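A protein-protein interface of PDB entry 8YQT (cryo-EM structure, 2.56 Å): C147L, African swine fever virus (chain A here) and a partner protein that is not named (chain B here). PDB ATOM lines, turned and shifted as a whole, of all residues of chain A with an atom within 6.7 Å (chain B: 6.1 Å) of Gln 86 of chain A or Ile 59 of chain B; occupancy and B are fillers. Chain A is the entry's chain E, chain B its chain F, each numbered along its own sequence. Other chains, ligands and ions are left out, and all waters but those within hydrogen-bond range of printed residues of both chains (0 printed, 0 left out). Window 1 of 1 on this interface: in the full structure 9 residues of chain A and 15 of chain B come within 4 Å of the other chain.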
ATOM      1  N   ARG A  78     -14.176   1.472 -21.024  1.00  0.00           N
ATOM      2  CA  ARG A  78     -15.567   1.871 -20.839  1.00  0.00           C
ATOM      3  C   ARG A  78     -16.266   0.995 -19.809  1.00  0.00           C
ATOM      4  O   ARG A  78     -17.017   1.498 -18.968  1.00  0.00           O
ATOM      5  CB  ARG A  78     -16.297   1.819 -22.180  1.00  0.00           C
ATOM      6  CG  ARG A  78     -17.779   2.115 -22.115  1.00  0.00           C
ATOM      7  CD  ARG A  78     -18.065   3.539 -21.682  1.00  0.00           C
ATOM      8  NE  ARG A  78     -19.482   3.851 -21.816  1.00  0.00           N
ATOM      9  CZ  ARG A  78     -20.079   4.896 -21.264  1.00  0.00           C
ATOM     10  NH1 ARG A  78     -19.410   5.762 -20.523  1.00  0.00           N
ATOM     11  NH2 ARG A  78     -21.382   5.076 -21.460  1.00  0.00           N
ATOM     12  N   ALA A  81     -14.949   1.980 -16.341  1.00  0.00           N
ATOM     13  CA  ALA A  81     -15.443   3.292 -15.931  1.00  0.00           C
ATOM     14  C   ALA A  81     -16.916   3.231 -15.545  1.00  0.00           C
ATOM     15  O   ALA A  81     -17.322   3.775 -14.508  1.00  0.00           O
ATOM     16  CB  ALA A  81     -15.223   4.309 -17.049  1.00  0.00           C
ATOM     17  N   VAL A  82     -17.728   2.561 -16.363  1.00  0.00           N
ATOM     18  CA  VAL A  82     -19.151   2.443 -16.069  1.00  0.00           C
ATOM     19  C   VAL A  82     -19.356   1.710 -14.754  1.00  0.00           C
ATOM     20  O   VAL A  82     -20.099   2.170 -13.882  1.00  0.00           O
ATOM     21  CB  VAL A  82     -19.885   1.743 -17.227  1.00  0.00           C
ATOM     22  CG1 VAL A  82     -21.254   1.266 -16.779  1.00  0.00           C
ATOM     23  CG2 VAL A  82     -20.014   2.676 -18.412  1.00  0.00           C
ATOM     24  N   ARG A  83     -18.675   0.574 -14.576  1.00  0.00           N
ATOM     25  CA  ARG A  83     -18.846  -0.212 -13.362  1.00  0.00           C
ATOM     26  C   ARG A  83     -18.357   0.533 -12.128  1.00  0.00           C
ATOM     27  O   ARG A  83     -18.969   0.426 -11.061  1.00  0.00           O
ATOM     28  CB  ARG A  83     -18.122  -1.548 -13.501  1.00  0.00           C
ATOM     29  CG  ARG A  83     -18.281  -2.453 -12.303  1.00  0.00           C
ATOM     30  CD  ARG A  83     -19.747  -2.705 -12.015  1.00  0.00           C
ATOM     31  NE  ARG A  83     -19.934  -3.468 -10.790  1.00  0.00           N
ATOM     32  CZ  ARG A  83     -21.096  -3.615 -10.172  1.00  0.00           C
ATOM     33  NH1 ARG A  83     -22.202  -3.066 -10.644  1.00  0.00           N
ATOM     34  NH2 ARG A  83     -21.151  -4.330  -9.054  1.00  0.00           N
ATOM     35  N   ALA A  84     -17.262   1.285 -12.247  1.00  0.00           N
ATOM     36  CA  ALA A  84     -16.787   2.089 -11.131  1.00  0.00           C
ATOM     37  C   ALA A  84     -17.789   3.166 -10.754  1.00  0.00           C
ATOM     38  O   ALA A  84     -17.989   3.434  -9.565  1.00  0.00           O
ATOM     39  CB  ALA A  84     -15.437   2.712 -11.476  1.00  0.00           C
ATOM     40  N   GLN A  85     -18.432   3.792 -11.741  1.00  0.00           N
ATOM     41  CA  GLN A  85     -19.488   4.747 -11.421  1.00  0.00           C
ATOM     42  C   GLN A  85     -20.690   4.068 -10.764  1.00  0.00           C
ATOM     43  O   GLN A  85     -21.275   4.623  -9.826  1.00  0.00           O
ATOM     44  CB  GLN A  85     -19.909   5.499 -12.681  1.00  0.00           C
ATOM     45  CG  GLN A  85     -20.861   6.642 -12.424  1.00  0.00           C
ATOM     46  CD  GLN A  85     -20.242   7.737 -11.593  1.00  0.00           C
ATOM     47  OE1 GLN A  85     -19.092   8.111 -11.800  1.00  0.00           O
ATOM     48  NE2 GLN A  85     -21.004   8.259 -10.643  1.00  0.00           N
ATOM     49  N   GLN A  86     -21.070   2.873 -11.230  1.00  0.00           N
ATOM     50  CA  GLN A  86     -22.153   2.143 -10.571  1.00  0.00           C
ATOM     51  C   GLN A  86     -21.811   1.859  -9.117  1.00  0.00           C
ATOM     52  O   GLN A  86     -22.656   2.016  -8.230  1.00  0.00           O
ATOM     53  CB  GLN A  86     -22.456   0.820 -11.279  1.00  0.00           C
ATOM     54  CG  GLN A  86     -22.430   0.826 -12.783  1.00  0.00           C
ATOM     55  CD  GLN A  86     -23.733   1.253 -13.394  1.00  0.00           C
ATOM     56  OE1 GLN A  86     -24.292   2.280 -13.028  1.00  0.00           O
ATOM     57  NE2 GLN A  86     -24.227   0.468 -14.339  1.00  0.00           N
ATOM     58  N   LEU A  87     -20.579   1.419  -8.858  1.00  0.00           N
ATOM     59  CA  LEU A  87     -20.157   1.147  -7.491  1.00  0.00           C
ATOM     60  C   LEU A  87     -20.128   2.414  -6.655  1.00  0.00           C
ATOM     61  O   LEU A  87     -20.440   2.374  -5.460  1.00  0.00           O
ATOM     62  CB  LEU A  87     -18.789   0.471  -7.489  1.00  0.00           C
ATOM     63  CG  LEU A  87     -18.779  -0.926  -8.103  1.00  0.00           C
ATOM     64  CD1 LEU A  87     -17.367  -1.345  -8.442  1.00  0.00           C
ATOM     65  CD2 LEU A  87     -19.425  -1.923  -7.161  1.00  0.00           C
ATOM     66  N   ALA A  88     -19.752   3.542  -7.255  1.00  0.00           N
ATOM     67  CA  ALA A  88     -19.891   4.820  -6.573  1.00  0.00           C
ATOM     68  C   ALA A  88     -21.349   5.156  -6.285  1.00  0.00           C
ATOM     69  O   ALA A  88     -21.621   5.945  -5.374  1.00  0.00           O
ATOM     70  CB  ALA A  88     -19.249   5.932  -7.399  1.00  0.00           C
ATOM     71  N   ILE A  89     -22.287   4.584  -7.040  1.00  0.00           N
ATOM     72  CA  ILE A  89     -23.704   4.785  -6.747  1.00  0.00           C
ATOM     73  C   ILE A  89     -24.177   3.831  -5.654  1.00  0.00           C
ATOM     74  O   ILE A  89     -24.755   4.258  -4.649  1.00  0.00           O
ATOM     75  CB  ILE A  89     -24.546   4.637  -8.028  1.00  0.00           C
ATOM     76  CG1 ILE A  89     -24.295   5.809  -8.977  1.00  0.00           C
ATOM     77  CG2 ILE A  89     -26.022   4.533  -7.688  1.00  0.00           C
ATOM     78  CD1 ILE A  89     -24.852   5.595 -10.368  1.00  0.00           C
ATOM     79  N   ASN A  90     -23.946   2.528  -5.828  1.00  0.00           N
ATOM     80  CA  ASN A  90     -24.415   1.520  -4.879  1.00  0.00           C
ATOM     81  C   ASN A  90     -23.327   1.042  -3.922  1.00  0.00           C
ATOM     82  O   ASN A  90     -23.464   1.177  -2.704  1.00  0.00           O
ATOM     83  CB  ASN A  90     -24.992   0.311  -5.625  1.00  0.00           C
ATOM     84  CG  ASN A  90     -26.496   0.346  -5.715  1.00  0.00           C
ATOM     85  OD1 ASN A  90     -27.168   0.889  -4.840  1.00  0.00           O
ATOM     86  ND2 ASN A  90     -27.039  -0.260  -6.761  1.00  0.00           N
ATOM     87  N   GLY A  91     -22.245   0.481  -4.454  1.00  0.00           N
ATOM     88  CA  GLY A  91     -21.257  -0.193  -3.641  1.00  0.00           C
ATOM     89  C   GLY A  91     -21.494  -1.676  -3.452  1.00  0.00           C
ATOM     90  O   GLY A  91     -20.725  -2.319  -2.729  1.00  0.00           O
ATOM     91  N   SER A  92     -22.524  -2.237  -4.079  1.00  0.00           N
ATOM     92  CA  SER A  92     -22.851  -3.653  -3.948  1.00  0.00           C
ATOM     93  C   SER A  92     -22.060  -4.443  -4.982  1.00  0.00           C
ATOM     94  O   SER A  92     -22.294  -4.312  -6.188  1.00  0.00           O
ATOM     95  CB  SER A  92     -24.351  -3.873  -4.126  1.00  0.00           C
ATOM     96  OG  SER A  92     -24.658  -5.254  -4.192  1.00  0.00           O
ATOM     97  N   PRO A 116     -20.961  -7.317 -14.051  1.00  0.00           N
ATOM     98  CA  PRO A 116     -22.350  -7.527 -14.473  1.00  0.00           C
ATOM     99  C   PRO A 116     -22.780  -6.634 -15.635  1.00  0.00           C
ATOM    100  O   PRO A 116     -23.828  -5.982 -15.591  1.00  0.00           O
ATOM    101  CB  PRO A 116     -23.134  -7.202 -13.200  1.00  0.00           C
ATOM    102  CG  PRO A 116     -22.335  -6.124 -12.581  1.00  0.00           C
ATOM    103  CD  PRO A 116     -20.886  -6.434 -12.876  1.00  0.00           C
ATOM    104  N   LEU A 117     -21.977  -6.606 -16.692  1.00  0.00           N
ATOM    105  CA  LEU A 117     -22.241  -5.764 -17.845  1.00  0.00           C
ATOM    106  C   LEU A 117     -22.135  -6.594 -19.115  1.00  0.00           C
ATOM    107  O   LEU A 117     -21.498  -7.648 -19.138  1.00  0.00           O
ATOM    108  CB  LEU A 117     -21.273  -4.577 -17.906  1.00  0.00           C
ATOM    109  CG  LEU A 117     -21.364  -3.569 -16.762  1.00  0.00           C
ATOM    110  CD1 LEU A 117     -20.288  -2.512 -16.882  1.00  0.00           C
ATOM    111  CD2 LEU A 117     -22.727  -2.929 -16.745  1.00  0.00           C
ATOM    112  N   ASP B  14     -31.827   5.534 -12.311  1.00  0.00           N
ATOM    113  CA  ASP B  14     -30.718   6.068 -11.533  1.00  0.00           C
ATOM    114  C   ASP B  14     -29.850   4.982 -10.912  1.00  0.00           C
ATOM    115  O   ASP B  14     -28.663   5.219 -10.674  1.00  0.00           O
ATOM    116  CB  ASP B  14     -31.254   6.992 -10.442  1.00  0.00           C
ATOM    117  CG  ASP B  14     -32.278   7.970 -10.969  1.00  0.00           C
ATOM    118  OD1 ASP B  14     -31.883   9.083 -11.374  1.00  0.00           O
ATOM    119  OD2 ASP B  14     -33.477   7.624 -10.989  1.00  0.00           O
ATOM    120  N   ASP B  15     -30.411   3.805 -10.649  1.00  0.00           N
ATOM    121  CA  ASP B  15     -29.673   2.705 -10.032  1.00  0.00           C
ATOM    122  C   ASP B  15     -29.879   1.456 -10.874  1.00  0.00           C
ATOM    123  O   ASP B  15     -30.710   0.600 -10.547  1.00  0.00           O
ATOM    124  CB  ASP B  15     -30.123   2.477  -8.591  1.00  0.00           C
ATOM    125  CG  ASP B  15     -29.124   1.680  -7.787  1.00  0.00           C
ATOM    126  OD1 ASP B  15     -29.199   1.723  -6.544  1.00  0.00           O
ATOM    127  OD2 ASP B  15     -28.263   1.010  -8.395  1.00  0.00           O
ATOM    128  N   PRO B  16     -29.140   1.322 -11.978  1.00  0.00           N
ATOM    129  CA  PRO B  16     -29.362   0.175 -12.871  1.00  0.00           C
ATOM    130  C   PRO B  16     -29.145  -1.172 -12.205  1.00  0.00           C
ATOM    131  O   PRO B  16     -29.870  -2.125 -12.516  1.00  0.00           O
ATOM    132  CB  PRO B  16     -28.352   0.414 -14.002  1.00  0.00           C
ATOM    133  CG  PRO B  16     -28.042   1.864 -13.934  1.00  0.00           C
ATOM    134  CD  PRO B  16     -28.092   2.218 -12.490  1.00  0.00           C
ATOM    135  N   THR B  17     -28.177  -1.278 -11.294  1.00  0.00           N
ATOM    136  CA  THR B  17     -27.908  -2.556 -10.645  1.00  0.00           C
ATOM    137  C   THR B  17     -29.092  -3.009  -9.801  1.00  0.00           C
ATOM    138  O   THR B  17     -29.527  -4.162  -9.897  1.00  0.00           O
ATOM    139  CB  THR B  17     -26.652  -2.451  -9.785  1.00  0.00           C
ATOM    140  OG1 THR B  17     -25.672  -1.655 -10.463  1.00  0.00           O
ATOM    141  CG2 THR B  17     -26.077  -3.827  -9.525  1.00  0.00           C
ATOM    142  N   CYS B  57     -31.466  -2.480 -20.602  1.00  0.00           N
ATOM    143  CA  CYS B  57     -31.105  -1.284 -19.848  1.00  0.00           C
ATOM    144  C   CYS B  57     -29.796  -0.743 -20.405  1.00  0.00           C
ATOM    145  O   CYS B  57     -28.713  -1.190 -20.026  1.00  0.00           O
ATOM    146  CB  CYS B  57     -30.991  -1.595 -18.360  1.00  0.00           C
ATOM    147  SG  CYS B  57     -30.598  -0.160 -17.337  1.00  0.00           S
ATOM    148  N   PHE B  58     -29.892   0.219 -21.316  1.00  0.00           N
ATOM    149  CA  PHE B  58     -28.708   0.874 -21.845  1.00  0.00           C
ATOM    150  C   PHE B  58     -28.127   1.824 -20.809  1.00  0.00           C
ATOM    151  O   PHE B  58     -28.847   2.406 -20.000  1.00  0.00           O
ATOM    152  CB  PHE B  58     -29.035   1.660 -23.112  1.00  0.00           C
ATOM    153  CG  PHE B  58     -29.720   0.861 -24.172  1.00  0.00           C
ATOM    154  CD1 PHE B  58     -29.021  -0.057 -24.926  1.00  0.00           C
ATOM    155  CD2 PHE B  58     -31.062   1.051 -24.438  1.00  0.00           C
ATOM    156  CE1 PHE B  58     -29.648  -0.783 -25.907  1.00  0.00           C
ATOM    157  CE2 PHE B  58     -31.693   0.328 -25.421  1.00  0.00           C
ATOM    158  CZ  PHE B  58     -30.985  -0.590 -26.156  1.00  0.00           C
ATOM    159  N   ILE B  59     -26.818   1.988 -20.849  1.00  0.00           N
ATOM    160  CA  ILE B  59     -26.136   2.965 -20.010  1.00  0.00           C
ATOM    161  C   ILE B  59     -26.024   4.269 -20.783  1.00  0.00           C
ATOM    162  O   ILE B  59     -25.689   4.273 -21.972  1.00  0.00           O
ATOM    163  CB  ILE B  59     -24.753   2.449 -19.571  1.00  0.00           C
ATOM    164  CG1 ILE B  59     -24.892   1.099 -18.867  1.00  0.00           C
ATOM    165  CG2 ILE B  59     -24.077   3.449 -18.659  1.00  0.00           C
ATOM    166  CD1 ILE B  59     -25.769   1.138 -17.646  1.00  0.00           C
ATOM    167  N   MET B  60     -26.326   5.380 -20.114  1.00  0.00           N
ATOM    168  CA  MET B  60     -26.285   6.682 -20.763  1.00  0.00           C
ATOM    169  C   MET B  60     -24.889   6.979 -21.289  1.00  0.00           C
ATOM    170  O   MET B  60     -23.886   6.737 -20.614  1.00  0.00           O
ATOM    171  CB  MET B  60     -26.728   7.773 -19.794  1.00  0.00           C
ATOM    172  CG  MET B  60     -28.218   7.788 -19.536  1.00  0.00           C
ATOM    173  SD  MET B  60     -28.740   9.178 -18.526  1.00  0.00           S
ATOM    174  CE  MET B  60     -30.198   8.489 -17.758  1.00  0.00           C
ATOM    175  N   ARG B  61     -24.832   7.519 -22.504  1.00  0.00           N
ATOM    176  CA  ARG B  61     -23.589   7.629 -23.248  1.00  0.00           C
ATOM    177  C   ARG B  61     -23.039   9.045 -23.324  1.00  0.00           C
ATOM    178  O   ARG B  61     -21.853   9.209 -23.615  1.00  0.00           O
ATOM    179  CB  ARG B  61     -23.792   7.099 -24.672  1.00  0.00           C
ATOM    180  CG  ARG B  61     -22.554   6.540 -25.329  1.00  0.00           C
ATOM    181  CD  ARG B  61     -22.593   6.775 -26.828  1.00  0.00           C
ATOM    182  NE  ARG B  61     -22.058   8.082 -27.190  1.00  0.00           N
ATOM    183  CZ  ARG B  61     -22.670   8.952 -27.983  1.00  0.00           C
ATOM    184  NH1 ARG B  61     -23.851   8.691 -28.514  1.00  0.00           N
ATOM    185  NH2 ARG B  61     -22.081  10.113 -28.245  1.00  0.00           N
ATOM    186  N   SER B  65     -22.573   9.930 -15.614  1.00  0.00           N
ATOM    187  CA  SER B  65     -23.374   9.625 -14.439  1.00  0.00           C
ATOM    188  C   SER B  65     -23.503   8.136 -14.170  1.00  0.00           C
ATOM    189  O   SER B  65     -23.844   7.755 -13.047  1.00  0.00           O
ATOM    190  CB  SER B  65     -24.770  10.235 -14.582  1.00  0.00           C
ATOM    191  OG  SER B  65     -25.419   9.755 -15.742  1.00  0.00           O
ATOM    192  N   GLY B  66     -23.243   7.289 -15.163  1.00  0.00           N
ATOM    193  CA  GLY B  66     -23.415   5.863 -14.990  1.00  0.00           C
ATOM    194  C   GLY B  66     -24.851   5.407 -14.986  1.00  0.00           C
ATOM    195  O   GLY B  66     -25.115   4.228 -14.740  1.00  0.00           O
ATOM    196  N   ARG B  67     -25.785   6.304 -15.264  1.00  0.00           N
ATOM    197  CA  ARG B  67     -27.207   6.031 -15.193  1.00  0.00           C
ATOM    198  C   ARG B  67     -27.664   5.288 -16.440  1.00  0.00           C
ATOM    199  O   ARG B  67     -27.053   5.376 -17.505  1.00  0.00           O
ATOM    200  CB  ARG B  67     -27.985   7.336 -15.033  1.00  0.00           C
ATOM    201  CG  ARG B  67     -28.205   7.736 -13.594  1.00  0.00           C
ATOM    202  CD  ARG B  67     -28.389   9.231 -13.449  1.00  0.00           C
ATOM    203  NE  ARG B  67     -29.682   9.685 -13.945  1.00  0.00           N
ATOM    204  CZ  ARG B  67     -29.841  10.611 -14.879  1.00  0.00           C
ATOM    205  NH1 ARG B  67     -28.804  11.210 -15.442  1.00  0.00           N
ATOM    206  NH2 ARG B  67     -31.070  10.950 -15.255  1.00  0.00           N
ATOM    207  N   GLY B  68     -28.754   4.539 -16.288  1.00  0.00           N
ATOM    208  CA  GLY B  68     -29.310   3.750 -17.360  1.00  0.00           C
ATOM    209  C   GLY B  68     -30.581   4.360 -17.927  1.00  0.00           C
ATOM    210  O   GLY B  68     -31.138   5.319 -17.405  1.00  0.00           O
ATOM    211  N   TYR B  69     -31.041   3.768 -19.023  1.00  0.00           N
ATOM    212  CA  TYR B  69     -32.320   4.154 -19.598  1.00  0.00           C
ATOM    213  C   TYR B  69     -32.887   2.962 -20.350  1.00  0.00           C
ATOM    214  O   TYR B  69     -32.156   2.063 -20.767  1.00  0.00           O
ATOM    215  CB  TYR B  69     -32.187   5.380 -20.507  1.00  0.00           C
ATOM    216  CG  TYR B  69     -31.430   5.141 -21.790  1.00  0.00           C
ATOM    217  CD1 TYR B  69     -30.049   5.246 -21.831  1.00  0.00           C
ATOM    218  CD2 TYR B  69     -32.097   4.832 -22.963  1.00  0.00           C
ATOM    219  CE1 TYR B  69     -29.357   5.040 -23.001  1.00  0.00           C
ATOM    220  CE2 TYR B  69     -31.414   4.622 -24.132  1.00  0.00           C
ATOM    221  CZ  TYR B  69     -30.044   4.727 -24.149  1.00  0.00           C
ATOM    222  OH  TYR B  69     -29.361   4.516 -25.322  1.00  0.00           O
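The side-chain amide oxygen (OE1) of Gln 86 of chain A sits close to the backbone carbonyl oxygen (O) of Gly 66 of chain B (2.7 Å).
The side-chain amide nitrogen (ND2) of Asn 90 of chain A lies within hydrogen-bond range of the side-chain carboxylate (OD2) of Asp 15 of chain B, at 2.4 Å.
The backbone carbonyl oxygen of Met 60 of chain B lies within hydrogen-bond range of the guanidinium group of Arg 78 of chain A.
The backbone carbonyl oxygen (O) of Ser 92 of chain A sits at hydrogen-bond distance from the guanidinium group (NH2) of Arg 83 of chain A, at 3.1 Å.
OD1 of Asp 14 of chain B is in salt-bridge range of NE of Arg 67 of chain B.
The backbone carbonyl oxygen (O) of Arg 67 of chain B lies within hydrogen-bond range of the backbone NH (N) of Met 60 of chain B (2.7 Å).
Arg 61 of chain B touches Arg 78 of chain A (CA to NH2, 3.8 Å).
Arg 83 of chain A touches Thr 17 of chain B (NH1 to OG1, 3.8 Å).
O of Ser 65 of chain B touches CG of Gln 85 of chain A (3.2 Å).
Gly 66 of chain B touches Gln 85 of chain A.
OE1 of Gln 86 of chain A touches CD of Pro 16 of chain B (3.8 Å).
CD1 of Ile 59 of chain B touches NE2 of Gln 86 of chain A, at 3.7 Å.
Ile 89 of chain A touches Asp 14 of chain B (CD1 to O, 3.8 Å).
CD1 of Ile 89 of chain A touches O of Ser 65 of chain B, at 3.6 Å.
Asn 90 of chain A touches Thr 17 of chain B (ND2 to CB, 3.8 Å).
Gln 86 of chain A touches three residues of chain B.
Of the printed residues of chain A, Ile 59 of chain B touches Gln 86 (3.7 Å).
Printed residues of chain A within 4 Å of Met 60 of chain B: Arg 78.
Of the printed residues of chain B, Gln 85 of chain A touches Ser 65 (3.2 Å) and Gly 66 (3.7 Å).
Of the printed residues of chain A, Arg 61 of chain B touches Arg 78 (3.8 Å).
Leu 117 of chain A touches none of the printed residues of chain B.
Gly 68 of chain B touches none of the printed residues of chain A.
The nearest residue of chain A that does not touch Ile 59 of chain B is Val 82 of chain A (4.03 Å).
Of the 14 printed residues of chain B, 9 touch a printed residue of chain A.
Of the 15 printed residues of chain A, 6 touch a printed residue of chain B.
Among the printed residues, 12 pairs touch across the chains.
Among the printed residues, no Asp or Glu carboxylate lies within 4 Å of a Lys or Arg side-chain nitrogen of the other chain.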
